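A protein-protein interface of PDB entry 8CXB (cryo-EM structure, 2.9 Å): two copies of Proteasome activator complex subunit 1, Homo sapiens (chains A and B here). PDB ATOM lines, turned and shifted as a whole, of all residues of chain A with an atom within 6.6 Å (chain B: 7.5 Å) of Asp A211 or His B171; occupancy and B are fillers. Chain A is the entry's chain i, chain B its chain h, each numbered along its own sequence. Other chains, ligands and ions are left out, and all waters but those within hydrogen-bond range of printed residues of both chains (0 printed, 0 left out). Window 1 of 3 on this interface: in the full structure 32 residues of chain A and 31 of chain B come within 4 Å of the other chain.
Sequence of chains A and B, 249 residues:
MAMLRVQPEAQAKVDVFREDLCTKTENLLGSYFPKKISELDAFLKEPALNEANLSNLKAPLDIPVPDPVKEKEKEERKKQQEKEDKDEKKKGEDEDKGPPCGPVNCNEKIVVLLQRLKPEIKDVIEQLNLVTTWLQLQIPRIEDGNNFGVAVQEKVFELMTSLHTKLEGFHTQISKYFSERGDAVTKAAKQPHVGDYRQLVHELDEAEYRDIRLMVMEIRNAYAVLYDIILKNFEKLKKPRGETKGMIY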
ATOM      1  N   LEU A 117      -6.219   1.501   6.274  1.00  0.00           N
ATOM      2  CA  LEU A 117      -5.126   1.686   7.265  1.00  0.00           C
ATOM      3  C   LEU A 117      -5.626   1.629   8.706  1.00  0.00           C
ATOM      4  O   LEU A 117      -4.944   1.012   9.529  1.00  0.00           O
ATOM      5  CB  LEU A 117      -4.458   3.030   6.980  1.00  0.00           C
ATOM      6  CG  LEU A 117      -3.385   3.460   7.971  1.00  0.00           C
ATOM      7  CD1 LEU A 117      -2.137   2.615   7.799  1.00  0.00           C
ATOM      8  CD2 LEU A 117      -3.059   4.931   7.793  1.00  0.00           C
ATOM      9  N   PHE A 170       0.295   7.836  15.525  1.00  0.00           N
ATOM     10  CA  PHE A 170      -0.399   7.566  14.246  1.00  0.00           C
ATOM     11  C   PHE A 170      -1.896   7.669  14.488  1.00  0.00           C
ATOM     12  O   PHE A 170      -2.601   8.255  13.664  1.00  0.00           O
ATOM     13  CB  PHE A 170      -0.120   6.148  13.750  1.00  0.00           C
ATOM     14  CG  PHE A 170       1.288   5.882  13.293  1.00  0.00           C
ATOM     15  CD1 PHE A 170       2.166   6.921  13.044  1.00  0.00           C
ATOM     16  CD2 PHE A 170       1.727   4.585  13.098  1.00  0.00           C
ATOM     17  CE1 PHE A 170       3.458   6.668  12.619  1.00  0.00           C
ATOM     18  CE2 PHE A 170       3.019   4.333  12.670  1.00  0.00           C
ATOM     19  CZ  PHE A 170       3.881   5.375  12.433  1.00  0.00           C
ATOM     20  N   GLN A 173      -2.861  11.214  14.648  1.00  0.00           N
ATOM     21  CA  GLN A 173      -2.729  11.951  13.373  1.00  0.00           C
ATOM     22  C   GLN A 173      -3.979  11.691  12.552  1.00  0.00           C
ATOM     23  O   GLN A 173      -4.475  12.617  11.906  1.00  0.00           O
ATOM     24  CB  GLN A 173      -1.480  11.500  12.624  1.00  0.00           C
ATOM     25  CG  GLN A 173      -1.401  12.022  11.200  1.00  0.00           C
ATOM     26  CD  GLN A 173      -1.247  13.520  11.160  1.00  0.00           C
ATOM     27  OE1 GLN A 173      -1.972  14.220  10.458  1.00  0.00           O
ATOM     28  NE2 GLN A 173      -0.298  14.024  11.932  1.00  0.00           N
ATOM     29  N   GLU A 206      -2.880  15.877   0.240  1.00  0.00           N
ATOM     30  CA  GLU A 206      -1.669  15.240  -0.319  1.00  0.00           C
ATOM     31  C   GLU A 206      -0.800  14.787   0.839  1.00  0.00           C
ATOM     32  O   GLU A 206      -0.304  13.658   0.804  1.00  0.00           O
ATOM     33  CB  GLU A 206      -0.863  16.245  -1.134  1.00  0.00           C
ATOM     34  CG  GLU A 206      -1.604  16.771  -2.345  1.00  0.00           C
ATOM     35  CD  GLU A 206      -0.765  17.660  -3.244  1.00  0.00           C
ATOM     36  OE1 GLU A 206       0.467  17.689  -3.055  1.00  0.00           O
ATOM     37  OE2 GLU A 206      -1.344  18.322  -4.127  1.00  0.00           O
ATOM     38  N   ALA A 207      -0.672  15.634   1.847  1.00  0.00           N
ATOM     39  CA  ALA A 207       0.232  15.299   2.959  1.00  0.00           C
ATOM     40  C   ALA A 207      -0.285  14.037   3.620  1.00  0.00           C
ATOM     41  O   ALA A 207       0.520  13.166   3.937  1.00  0.00           O
ATOM     42  CB  ALA A 207       0.235  16.428   3.937  1.00  0.00           C
ATOM     43  N   GLU A 208      -1.597  13.956   3.788  1.00  0.00           N
ATOM     44  CA  GLU A 208      -2.180  12.789   4.476  1.00  0.00           C
ATOM     45  C   GLU A 208      -1.840  11.560   3.649  1.00  0.00           C
ATOM     46  O   GLU A 208      -1.483  10.544   4.241  1.00  0.00           O
ATOM     47  CB  GLU A 208      -3.690  12.943   4.611  1.00  0.00           C
ATOM     48  CG  GLU A 208      -4.354  11.777   5.318  1.00  0.00           C
ATOM     49  CD  GLU A 208      -3.995  11.607   6.784  1.00  0.00           C
ATOM     50  OE1 GLU A 208      -3.541  12.586   7.402  1.00  0.00           O
ATOM     51  OE2 GLU A 208      -4.172  10.491   7.307  1.00  0.00           O
ATOM     52  N   TYR A 209      -1.921  11.669   2.327  1.00  0.00           N
ATOM     53  CA  TYR A 209      -1.676  10.465   1.510  1.00  0.00           C
ATOM     54  C   TYR A 209      -0.253  10.029   1.784  1.00  0.00           C
ATOM     55  O   TYR A 209      -0.012   8.844   2.035  1.00  0.00           O
ATOM     56  CB  TYR A 209      -1.685  10.846   0.038  1.00  0.00           C
ATOM     57  CG  TYR A 209      -1.418   9.720  -0.923  1.00  0.00           C
ATOM     58  CD1 TYR A 209      -2.421   8.832  -1.262  1.00  0.00           C
ATOM     59  CD2 TYR A 209      -0.174   9.557  -1.509  1.00  0.00           C
ATOM     60  CE1 TYR A 209      -2.195   7.799  -2.152  1.00  0.00           C
ATOM     61  CE2 TYR A 209       0.070   8.527  -2.399  1.00  0.00           C
ATOM     62  CZ  TYR A 209      -0.946   7.647  -2.719  1.00  0.00           C
ATOM     63  OH  TYR A 209      -0.730   6.630  -3.596  1.00  0.00           O
ATOM     64  N   ARG A 210       0.653  10.993   1.779  1.00  0.00           N
ATOM     65  CA  ARG A 210       2.073  10.642   1.971  1.00  0.00           C
ATOM     66  C   ARG A 210       2.254  10.055   3.369  1.00  0.00           C
ATOM     67  O   ARG A 210       2.929   9.029   3.493  1.00  0.00           O
ATOM     68  CB  ARG A 210       2.920  11.880   1.693  1.00  0.00           C
ATOM     69  CG  ARG A 210       2.723  12.448   0.295  1.00  0.00           C
ATOM     70  CD  ARG A 210       3.253  13.865   0.200  1.00  0.00           C
ATOM     71  NE  ARG A 210       3.258  14.469  -1.125  1.00  0.00           N
ATOM     72  CZ  ARG A 210       4.235  14.337  -2.014  1.00  0.00           C
ATOM     73  NH1 ARG A 210       5.292  13.594  -1.739  1.00  0.00           N
ATOM     74  NH2 ARG A 210       4.148  14.942  -3.184  1.00  0.00           N
ATOM     75  N   ASP A 211       1.627  10.661   4.370  1.00  0.00           N
ATOM     76  CA  ASP A 211       1.787  10.169   5.759  1.00  0.00           C
ATOM     77  C   ASP A 211       1.213   8.765   5.852  1.00  0.00           C
ATOM     78  O   ASP A 211       1.833   7.925   6.496  1.00  0.00           O
ATOM     79  CB  ASP A 211       1.126  11.074   6.791  1.00  0.00           C
ATOM     80  CG  ASP A 211       1.877  12.372   7.014  1.00  0.00           C
ATOM     81  OD1 ASP A 211       2.831  12.630   6.257  1.00  0.00           O
ATOM     82  OD2 ASP A 211       1.502  13.109   7.945  1.00  0.00           O
ATOM     83  N   ILE A 212       0.078   8.531   5.211  1.00  0.00           N
ATOM     84  CA  ILE A 212      -0.567   7.194   5.286  1.00  0.00           C
ATOM     85  C   ILE A 212       0.420   6.198   4.689  1.00  0.00           C
ATOM     86  O   ILE A 212       0.596   5.120   5.269  1.00  0.00           O
ATOM     87  CB  ILE A 212      -1.899   7.194   4.519  1.00  0.00           C
ATOM     88  CG1 ILE A 212      -3.010   7.910   5.287  1.00  0.00           C
ATOM     89  CG2 ILE A 212      -2.316   5.784   4.135  1.00  0.00           C
ATOM     90  CD1 ILE A 212      -4.266   8.080   4.476  1.00  0.00           C
ATOM     91  N   ARG A 213       1.079   6.574   3.596  1.00  0.00           N
ATOM     92  CA  ARG A 213       1.976   5.600   2.935  1.00  0.00           C
ATOM     93  C   ARG A 213       3.075   5.243   3.929  1.00  0.00           C
ATOM     94  O   ARG A 213       3.352   4.048   4.098  1.00  0.00           O
ATOM     95  CB  ARG A 213       2.520   6.169   1.623  1.00  0.00           C
ATOM     96  CG  ARG A 213       4.036   6.193   1.506  1.00  0.00           C
ATOM     97  CD  ARG A 213       4.482   5.893   0.091  1.00  0.00           C
ATOM     98  NE  ARG A 213       4.143   4.524  -0.257  1.00  0.00           N
ATOM     99  CZ  ARG A 213       4.452   3.944  -1.408  1.00  0.00           C
ATOM    100  NH1 ARG A 213       5.114   4.620  -2.331  1.00  0.00           N
ATOM    101  NH2 ARG A 213       4.102   2.691  -1.631  1.00  0.00           N
ATOM    102  N   LEU A 214       3.618   6.244   4.614  1.00  0.00           N
ATOM    103  CA  LEU A 214       4.695   5.981   5.589  1.00  0.00           C
ATOM    104  C   LEU A 214       4.126   5.111   6.697  1.00  0.00           C
ATOM    105  O   LEU A 214       4.811   4.186   7.128  1.00  0.00           O
ATOM    106  CB  LEU A 214       5.175   7.312   6.160  1.00  0.00           C
ATOM    107  CG  LEU A 214       5.713   8.304   5.134  1.00  0.00           C
ATOM    108  CD1 LEU A 214       5.959   9.661   5.773  1.00  0.00           C
ATOM    109  CD2 LEU A 214       6.981   7.774   4.484  1.00  0.00           C
ATOM    110  N   MET A 215       2.902   5.395   7.121  1.00  0.00           N
ATOM    111  CA  MET A 215       2.378   4.638   8.272  1.00  0.00           C
ATOM    112  C   MET A 215       2.345   3.181   7.863  1.00  0.00           C
ATOM    113  O   MET A 215       2.770   2.353   8.656  1.00  0.00           O
ATOM    114  CB  MET A 215       0.963   5.073   8.634  1.00  0.00           C
ATOM    115  CG  MET A 215       0.913   6.408   9.333  1.00  0.00           C
ATOM    116  SD  MET A 215      -0.729   6.763   9.987  1.00  0.00           S
ATOM    117  CE  MET A 215      -0.525   8.477  10.463  1.00  0.00           C
ATOM    118  N   VAL A 216       1.906   2.892   6.650  1.00  0.00           N
ATOM    119  CA  VAL A 216       1.786   1.454   6.307  1.00  0.00           C
ATOM    120  C   VAL A 216       3.188   0.861   6.377  1.00  0.00           C
ATOM    121  O   VAL A 216       3.342  -0.242   6.918  1.00  0.00           O
ATOM    122  CB  VAL A 216       1.149   1.250   4.927  1.00  0.00           C
ATOM    123  CG1 VAL A 216       1.006  -0.224   4.592  1.00  0.00           C
ATOM    124  CG2 VAL A 216      -0.194   1.948   4.823  1.00  0.00           C
ATOM    125  N   GLU A 218       5.741   1.825   8.148  1.00  0.00           N
ATOM    126  CA  GLU A 218       6.200   1.743   9.556  1.00  0.00           C
ATOM    127  C   GLU A 218       5.462   0.616  10.267  1.00  0.00           C
ATOM    128  O   GLU A 218       6.085  -0.072  11.067  1.00  0.00           O
ATOM    129  CB  GLU A 218       5.999   3.079  10.255  1.00  0.00           C
ATOM    130  CG  GLU A 218       6.851   4.188   9.672  1.00  0.00           C
ATOM    131  CD  GLU A 218       6.810   5.495  10.441  1.00  0.00           C
ATOM    132  OE1 GLU A 218       6.416   6.519   9.846  1.00  0.00           O
ATOM    133  OE2 GLU A 218       7.181   5.489  11.631  1.00  0.00           O
ATOM    134  N   LYS B 118       8.579  19.441  -2.256  1.00  0.00           N
ATOM    135  CA  LYS B 118       7.744  18.522  -1.446  1.00  0.00           C
ATOM    136  C   LYS B 118       8.028  17.061  -1.776  1.00  0.00           C
ATOM    137  O   LYS B 118       8.180  16.288  -0.827  1.00  0.00           O
ATOM    138  CB  LYS B 118       6.255  18.804  -1.635  1.00  0.00           C
ATOM    139  CG  LYS B 118       5.633  19.776  -0.645  1.00  0.00           C
ATOM    140  CD  LYS B 118       4.128  19.669  -0.635  1.00  0.00           C
ATOM    141  CE  LYS B 118       3.656  18.243  -0.439  1.00  0.00           C
ATOM    142  NZ  LYS B 118       2.181  18.131  -0.519  1.00  0.00           N
ATOM    143  N   ILE B 121      11.225  15.897   0.028  1.00  0.00           N
ATOM    144  CA  ILE B 121      11.199  15.739   1.507  1.00  0.00           C
ATOM    145  C   ILE B 121      10.572  14.387   1.797  1.00  0.00           C
ATOM    146  O   ILE B 121      11.093  13.653   2.631  1.00  0.00           O
ATOM    147  CB  ILE B 121      10.384  16.855   2.175  1.00  0.00           C
ATOM    148  CG1 ILE B 121      10.894  18.246   1.801  1.00  0.00           C
ATOM    149  CG2 ILE B 121      10.341  16.668   3.683  1.00  0.00           C
ATOM    150  CD1 ILE B 121      11.752  18.879   2.865  1.00  0.00           C
ATOM    151  N   LYS B 122       9.488  14.067   1.112  1.00  0.00           N
ATOM    152  CA  LYS B 122       8.820  12.797   1.455  1.00  0.00           C
ATOM    153  C   LYS B 122       9.767  11.648   1.117  1.00  0.00           C
ATOM    154  O   LYS B 122       9.803  10.674   1.877  1.00  0.00           O
ATOM    155  CB  LYS B 122       7.427  12.742   0.834  1.00  0.00           C
ATOM    156  CG  LYS B 122       6.454  13.750   1.419  1.00  0.00           C
ATOM    157  CD  LYS B 122       6.299  13.621   2.914  1.00  0.00           C
ATOM    158  CE  LYS B 122       5.178  14.485   3.445  1.00  0.00           C
ATOM    159  NZ  LYS B 122       5.173  15.811   2.786  1.00  0.00           N
ATOM    160  N   ILE B 125      12.274  10.966   3.802  1.00  0.00           N
ATOM    161  CA  ILE B 125      11.690  10.363   5.023  1.00  0.00           C
ATOM    162  C   ILE B 125      11.540   8.876   4.750  1.00  0.00           C
ATOM    163  O   ILE B 125      11.925   8.084   5.608  1.00  0.00           O
ATOM    164  CB  ILE B 125      10.339  11.007   5.369  1.00  0.00           C
ATOM    165  CG1 ILE B 125      10.503  12.492   5.697  1.00  0.00           C
ATOM    166  CG2 ILE B 125       9.660  10.264   6.505  1.00  0.00           C
ATOM    167  CD1 ILE B 125       9.226  13.164   6.140  1.00  0.00           C
ATOM    168  N   THR B 165      13.818  13.534  12.481  1.00  0.00           N
ATOM    169  CA  THR B 165      13.101  14.610  13.195  1.00  0.00           C
ATOM    170  C   THR B 165      13.180  15.896  12.388  1.00  0.00           C
ATOM    171  O   THR B 165      12.141  16.540  12.217  1.00  0.00           O
ATOM    172  CB  THR B 165      13.738  14.860  14.558  1.00  0.00           C
ATOM    173  OG1 THR B 165      13.826  13.598  15.218  1.00  0.00           O
ATOM    174  CG2 THR B 165      12.955  15.835  15.407  1.00  0.00           C
ATOM    175  N   LYS B 166      14.360  16.233  11.882  1.00  0.00           N
ATOM    176  CA  LYS B 166      14.501  17.528  11.180  1.00  0.00           C
ATOM    177  C   LYS B 166      13.616  17.499   9.946  1.00  0.00           C
ATOM    178  O   LYS B 166      12.960  18.504   9.672  1.00  0.00           O
ATOM    179  CB  LYS B 166      15.951  17.747  10.763  1.00  0.00           C
ATOM    180  CG  LYS B 166      16.950  17.703  11.907  1.00  0.00           C
ATOM    181  CD  LYS B 166      18.383  17.882  11.469  1.00  0.00           C
ATOM    182  CE  LYS B 166      19.357  17.746  12.619  1.00  0.00           C
ATOM    183  NZ  LYS B 166      20.752  18.005  12.193  1.00  0.00           N
ATOM    184  N   LEU B 167      13.624  16.382   9.231  1.00  0.00           N
ATOM    185  CA  LEU B 167      12.808  16.253   8.002  1.00  0.00           C
ATOM    186  C   LEU B 167      11.329  16.281   8.354  1.00  0.00           C
ATOM    187  O   LEU B 167      10.563  16.886   7.606  1.00  0.00           O
ATOM    188  CB  LEU B 167      13.194  14.960   7.296  1.00  0.00           C
ATOM    189  CG  LEU B 167      14.670  14.892   6.926  1.00  0.00           C
ATOM    190  CD1 LEU B 167      15.062  13.482   6.546  1.00  0.00           C
ATOM    191  CD2 LEU B 167      15.006  15.878   5.821  1.00  0.00           C
ATOM    192  N   GLU B 168      10.944  15.656   9.456  1.00  0.00           N
ATOM    193  CA  GLU B 168       9.524  15.761   9.853  1.00  0.00           C
ATOM    194  C   GLU B 168       9.230  17.235  10.111  1.00  0.00           C
ATOM    195  O   GLU B 168       8.149  17.698   9.725  1.00  0.00           O
ATOM    196  CB  GLU B 168       9.244  14.915  11.091  1.00  0.00           C
ATOM    197  CG  GLU B 168       9.199  13.426  10.807  1.00  0.00           C
ATOM    198  CD  GLU B 168       7.976  12.963  10.035  1.00  0.00           C
ATOM    199  OE1 GLU B 168       6.946  13.665  10.084  1.00  0.00           O
ATOM    200  OE2 GLU B 168       8.056  11.902   9.384  1.00  0.00           O
ATOM    201  N   GLY B 169      10.172  17.942  10.726  1.00  0.00           N
ATOM    202  CA  GLY B 169       9.986  19.379  10.977  1.00  0.00           C
ATOM    203  C   GLY B 169       9.849  20.124   9.669  1.00  0.00           C
ATOM    204  O   GLY B 169       9.017  21.033   9.590  1.00  0.00           O
ATOM    205  N   PHE B 170      10.643  19.744   8.675  1.00  0.00           N
ATOM    206  CA  PHE B 170      10.600  20.446   7.377  1.00  0.00           C
ATOM    207  C   PHE B 170       9.196  20.253   6.825  1.00  0.00           C
ATOM    208  O   PHE B 170       8.610  21.204   6.299  1.00  0.00           O
ATOM    209  CB  PHE B 170      11.639  19.880   6.413  1.00  0.00           C
ATOM    210  CG  PHE B 170      13.049  20.339   6.660  1.00  0.00           C
ATOM    211  CD1 PHE B 170      13.301  21.518   7.335  1.00  0.00           C
ATOM    212  CD2 PHE B 170      14.123  19.598   6.199  1.00  0.00           C
ATOM    213  CE1 PHE B 170      14.601  21.942   7.558  1.00  0.00           C
ATOM    214  CE2 PHE B 170      15.421  20.023   6.421  1.00  0.00           C
ATOM    215  CZ  PHE B 170      15.657  21.193   7.101  1.00  0.00           C
ATOM    216  N   HIS B 171       8.662  19.050   6.986  1.00  0.00           N
ATOM    217  CA  HIS B 171       7.324  18.769   6.423  1.00  0.00           C
ATOM    218  C   HIS B 171       6.330  19.703   7.098  1.00  0.00           C
ATOM    219  O   HIS B 171       5.487  20.279   6.401  1.00  0.00           O
ATOM    220  CB  HIS B 171       6.981  17.293   6.615  1.00  0.00           C
ATOM    221  CG  HIS B 171       5.520  17.010   6.610  1.00  0.00           C
ATOM    222  ND1 HIS B 171       4.715  17.305   5.529  1.00  0.00           N
ATOM    223  CD2 HIS B 171       4.716  16.457   7.543  1.00  0.00           C
ATOM    224  CE1 HIS B 171       3.476  16.949   5.797  1.00  0.00           C
ATOM    225  NE2 HIS B 171       3.450  16.425   7.027  1.00  0.00           N
ATOM    226  N   THR B 172       6.458  19.873   8.406  1.00  0.00           N
ATOM    227  CA  THR B 172       5.497  20.721   9.141  1.00  0.00           C
ATOM    228  C   THR B 172       5.615  22.155   8.644  1.00  0.00           C
ATOM    229  O   THR B 172       4.584  22.797   8.448  1.00  0.00           O
ATOM    230  CB  THR B 172       5.795  20.679  10.638  1.00  0.00           C
ATOM    231  OG1 THR B 172       5.825  19.306  11.022  1.00  0.00           O
ATOM    232  CG2 THR B 172       4.771  21.423  11.466  1.00  0.00           C
ATOM    233  N   GLN B 173       6.836  22.623   8.421  1.00  0.00           N
ATOM    234  CA  GLN B 173       7.013  24.042   8.038  1.00  0.00           C
ATOM    235  C   GLN B 173       6.287  24.270   6.718  1.00  0.00           C
ATOM    236  O   GLN B 173       5.608  25.295   6.577  1.00  0.00           O
ATOM    237  CB  GLN B 173       8.501  24.357   7.929  1.00  0.00           C
ATOM    238  CG  GLN B 173       8.795  25.710   7.300  1.00  0.00           C
ATOM    239  CD  GLN B 173       8.288  26.853   8.142  1.00  0.00           C
ATOM    240  OE1 GLN B 173       7.603  27.751   7.657  1.00  0.00           O
ATOM    241  NE2 GLN B 173       8.620  26.824   9.423  1.00  0.00           N
ATOM    242  N   ILE B 174       6.395  23.311   5.810  1.00  0.00           N
ATOM    243  CA  ILE B 174       5.741  23.462   4.487  1.00  0.00           C
ATOM    244  C   ILE B 174       4.243  23.576   4.734  1.00  0.00           C
ATOM    245  O   ILE B 174       3.616  24.473   4.161  1.00  0.00           O
ATOM    246  CB  ILE B 174       6.046  22.227   3.628  1.00  0.00           C
ATOM    247  CG1 ILE B 174       7.522  22.162   3.233  1.00  0.00           C
ATOM    248  CG2 ILE B 174       5.134  22.168   2.415  1.00  0.00           C
ATOM    249  CD1 ILE B 174       7.916  20.872   2.562  1.00  0.00           C
ATOM    250  N   SER B 175       3.700  22.722   5.594  1.00  0.00           N
ATOM    251  CA  SER B 175       2.231  22.732   5.787  1.00  0.00           C
ATOM    252  C   SER B 175       1.798  24.056   6.402  1.00  0.00           C
ATOM    253  O   SER B 175       0.775  24.600   5.974  1.00  0.00           O
ATOM    254  CB  SER B 175       1.786  21.574   6.620  1.00  0.00           C
ATOM    255  OG  SER B 175       2.271  21.687   7.946  1.00  0.00           O
ATOM    256  N   LYS B 176       2.564  24.554   7.363  1.00  0.00           N
ATOM    257  CA  LYS B 176       2.134  25.779   8.072  1.00  0.00           C
ATOM    258  C   LYS B 176       2.119  26.965   7.118  1.00  0.00           C
ATOM    259  O   LYS B 176       1.291  27.853   7.316  1.00  0.00           O
ATOM    260  CB  LYS B 176       2.991  26.028   9.312  1.00  0.00           C
ATOM    261  CG  LYS B 176       4.114  27.041   9.165  1.00  0.00           C
ATOM    262  CD  LYS B 176       4.766  27.363  10.488  1.00  0.00           C
ATOM    263  CE  LYS B 176       5.733  28.524  10.405  1.00  0.00           C
ATOM    264  NZ  LYS B 176       6.062  29.059  11.748  1.00  0.00           N
ATOM    265  N   TYR B 177       2.966  26.967   6.097  1.00  0.00           N
ATOM    266  CA  TYR B 177       3.048  28.188   5.268  1.00  0.00           C
ATOM    267  C   TYR B 177       1.671  28.488   4.720  1.00  0.00           C
ATOM    268  O   TYR B 177       1.221  29.629   4.821  1.00  0.00           O
ATOM    269  CB  TYR B 177       3.903  27.932   4.035  1.00  0.00           C
ATOM    270  CG  TYR B 177       3.782  28.957   2.939  1.00  0.00           C
ATOM    271  CD1 TYR B 177       4.199  30.262   3.130  1.00  0.00           C
ATOM    272  CD2 TYR B 177       3.268  28.615   1.701  1.00  0.00           C
ATOM    273  CE1 TYR B 177       4.099  31.206   2.124  1.00  0.00           C
ATOM    274  CE2 TYR B 177       3.157  29.548   0.685  1.00  0.00           C
ATOM    275  CZ  TYR B 177       3.576  30.847   0.897  1.00  0.00           C
ATOM    276  OH  TYR B 177       3.472  31.767  -0.102  1.00  0.00           O
ATOM    277  N   MET B 215      15.843  24.002   3.012  1.00  0.00           N
ATOM    278  CA  MET B 215      15.459  22.582   3.135  1.00  0.00           C
ATOM    279  C   MET B 215      16.197  21.832   2.036  1.00  0.00           C
ATOM    280  O   MET B 215      16.739  20.767   2.324  1.00  0.00           O
ATOM    281  CB  MET B 215      13.958  22.382   2.953  1.00  0.00           C
ATOM    282  CG  MET B 215      13.132  23.043   4.023  1.00  0.00           C
ATOM    283  SD  MET B 215      11.397  22.578   3.902  1.00  0.00           S
ATOM    284  CE  MET B 215      10.618  24.087   4.471  1.00  0.00           C
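The side-chain amino group of Lys B118 lies within salt-bridge range of the side-chain carboxylate of Glu A206 (3.1 Å).
Of chain A, only Ala A207 (3.8 Å) and Asp A211 (3.9 Å) come within 4 Å of His B171.
Of the printed residues of chain B, Leu A214 touches Ile B125.
Printed residues of chain B within 4 Å of Arg A210: Lys B118 (3.9 Å) and Lys B122 (3.4 Å).
Of the printed residues of chain A, Lys B122 touches Arg A210.
Of the printed residues of chain A, Ile B125 touches Leu A214.
Of the printed residues of chain B, Ala A207 touches His B171 (3.8 Å).
Lys B166 touches none of the printed residues of chain A.
Leu B167 touches none of the printed residues of chain A.
The nearest residue of chain A that does not touch His B171 is Glu A208 (6.2 Å).
Printed residues of chain B that touch a printed residue of chain A: Lys B118, Lys B122, Ile B125 and His B171.
Among the printed residues, 6 pairs touch across the chains.
Among the printed residues, Asp or Glu carboxylates within 4 Å of a Lys or Arg side-chain nitrogen of the other chain: Glu A206 with Lys B118 (3.1 Å).
Among the printed residues, pairs that only touch across the chains: Ala A207 with His B171 (3.8 Å), Arg A210 with Lys B118 (3.9 Å), Arg A210 with Lys B122 (3.4 Å), Asp A211 with His B171 (3.9 Å) and Leu A214 with Ile B125 (3.8 Å).
Positions printed for both chains: 170, 173 and 215.
NZ of Lys B122 sits at hydrogen-bond distance from ND1 of His B171, 3.2 Å away.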
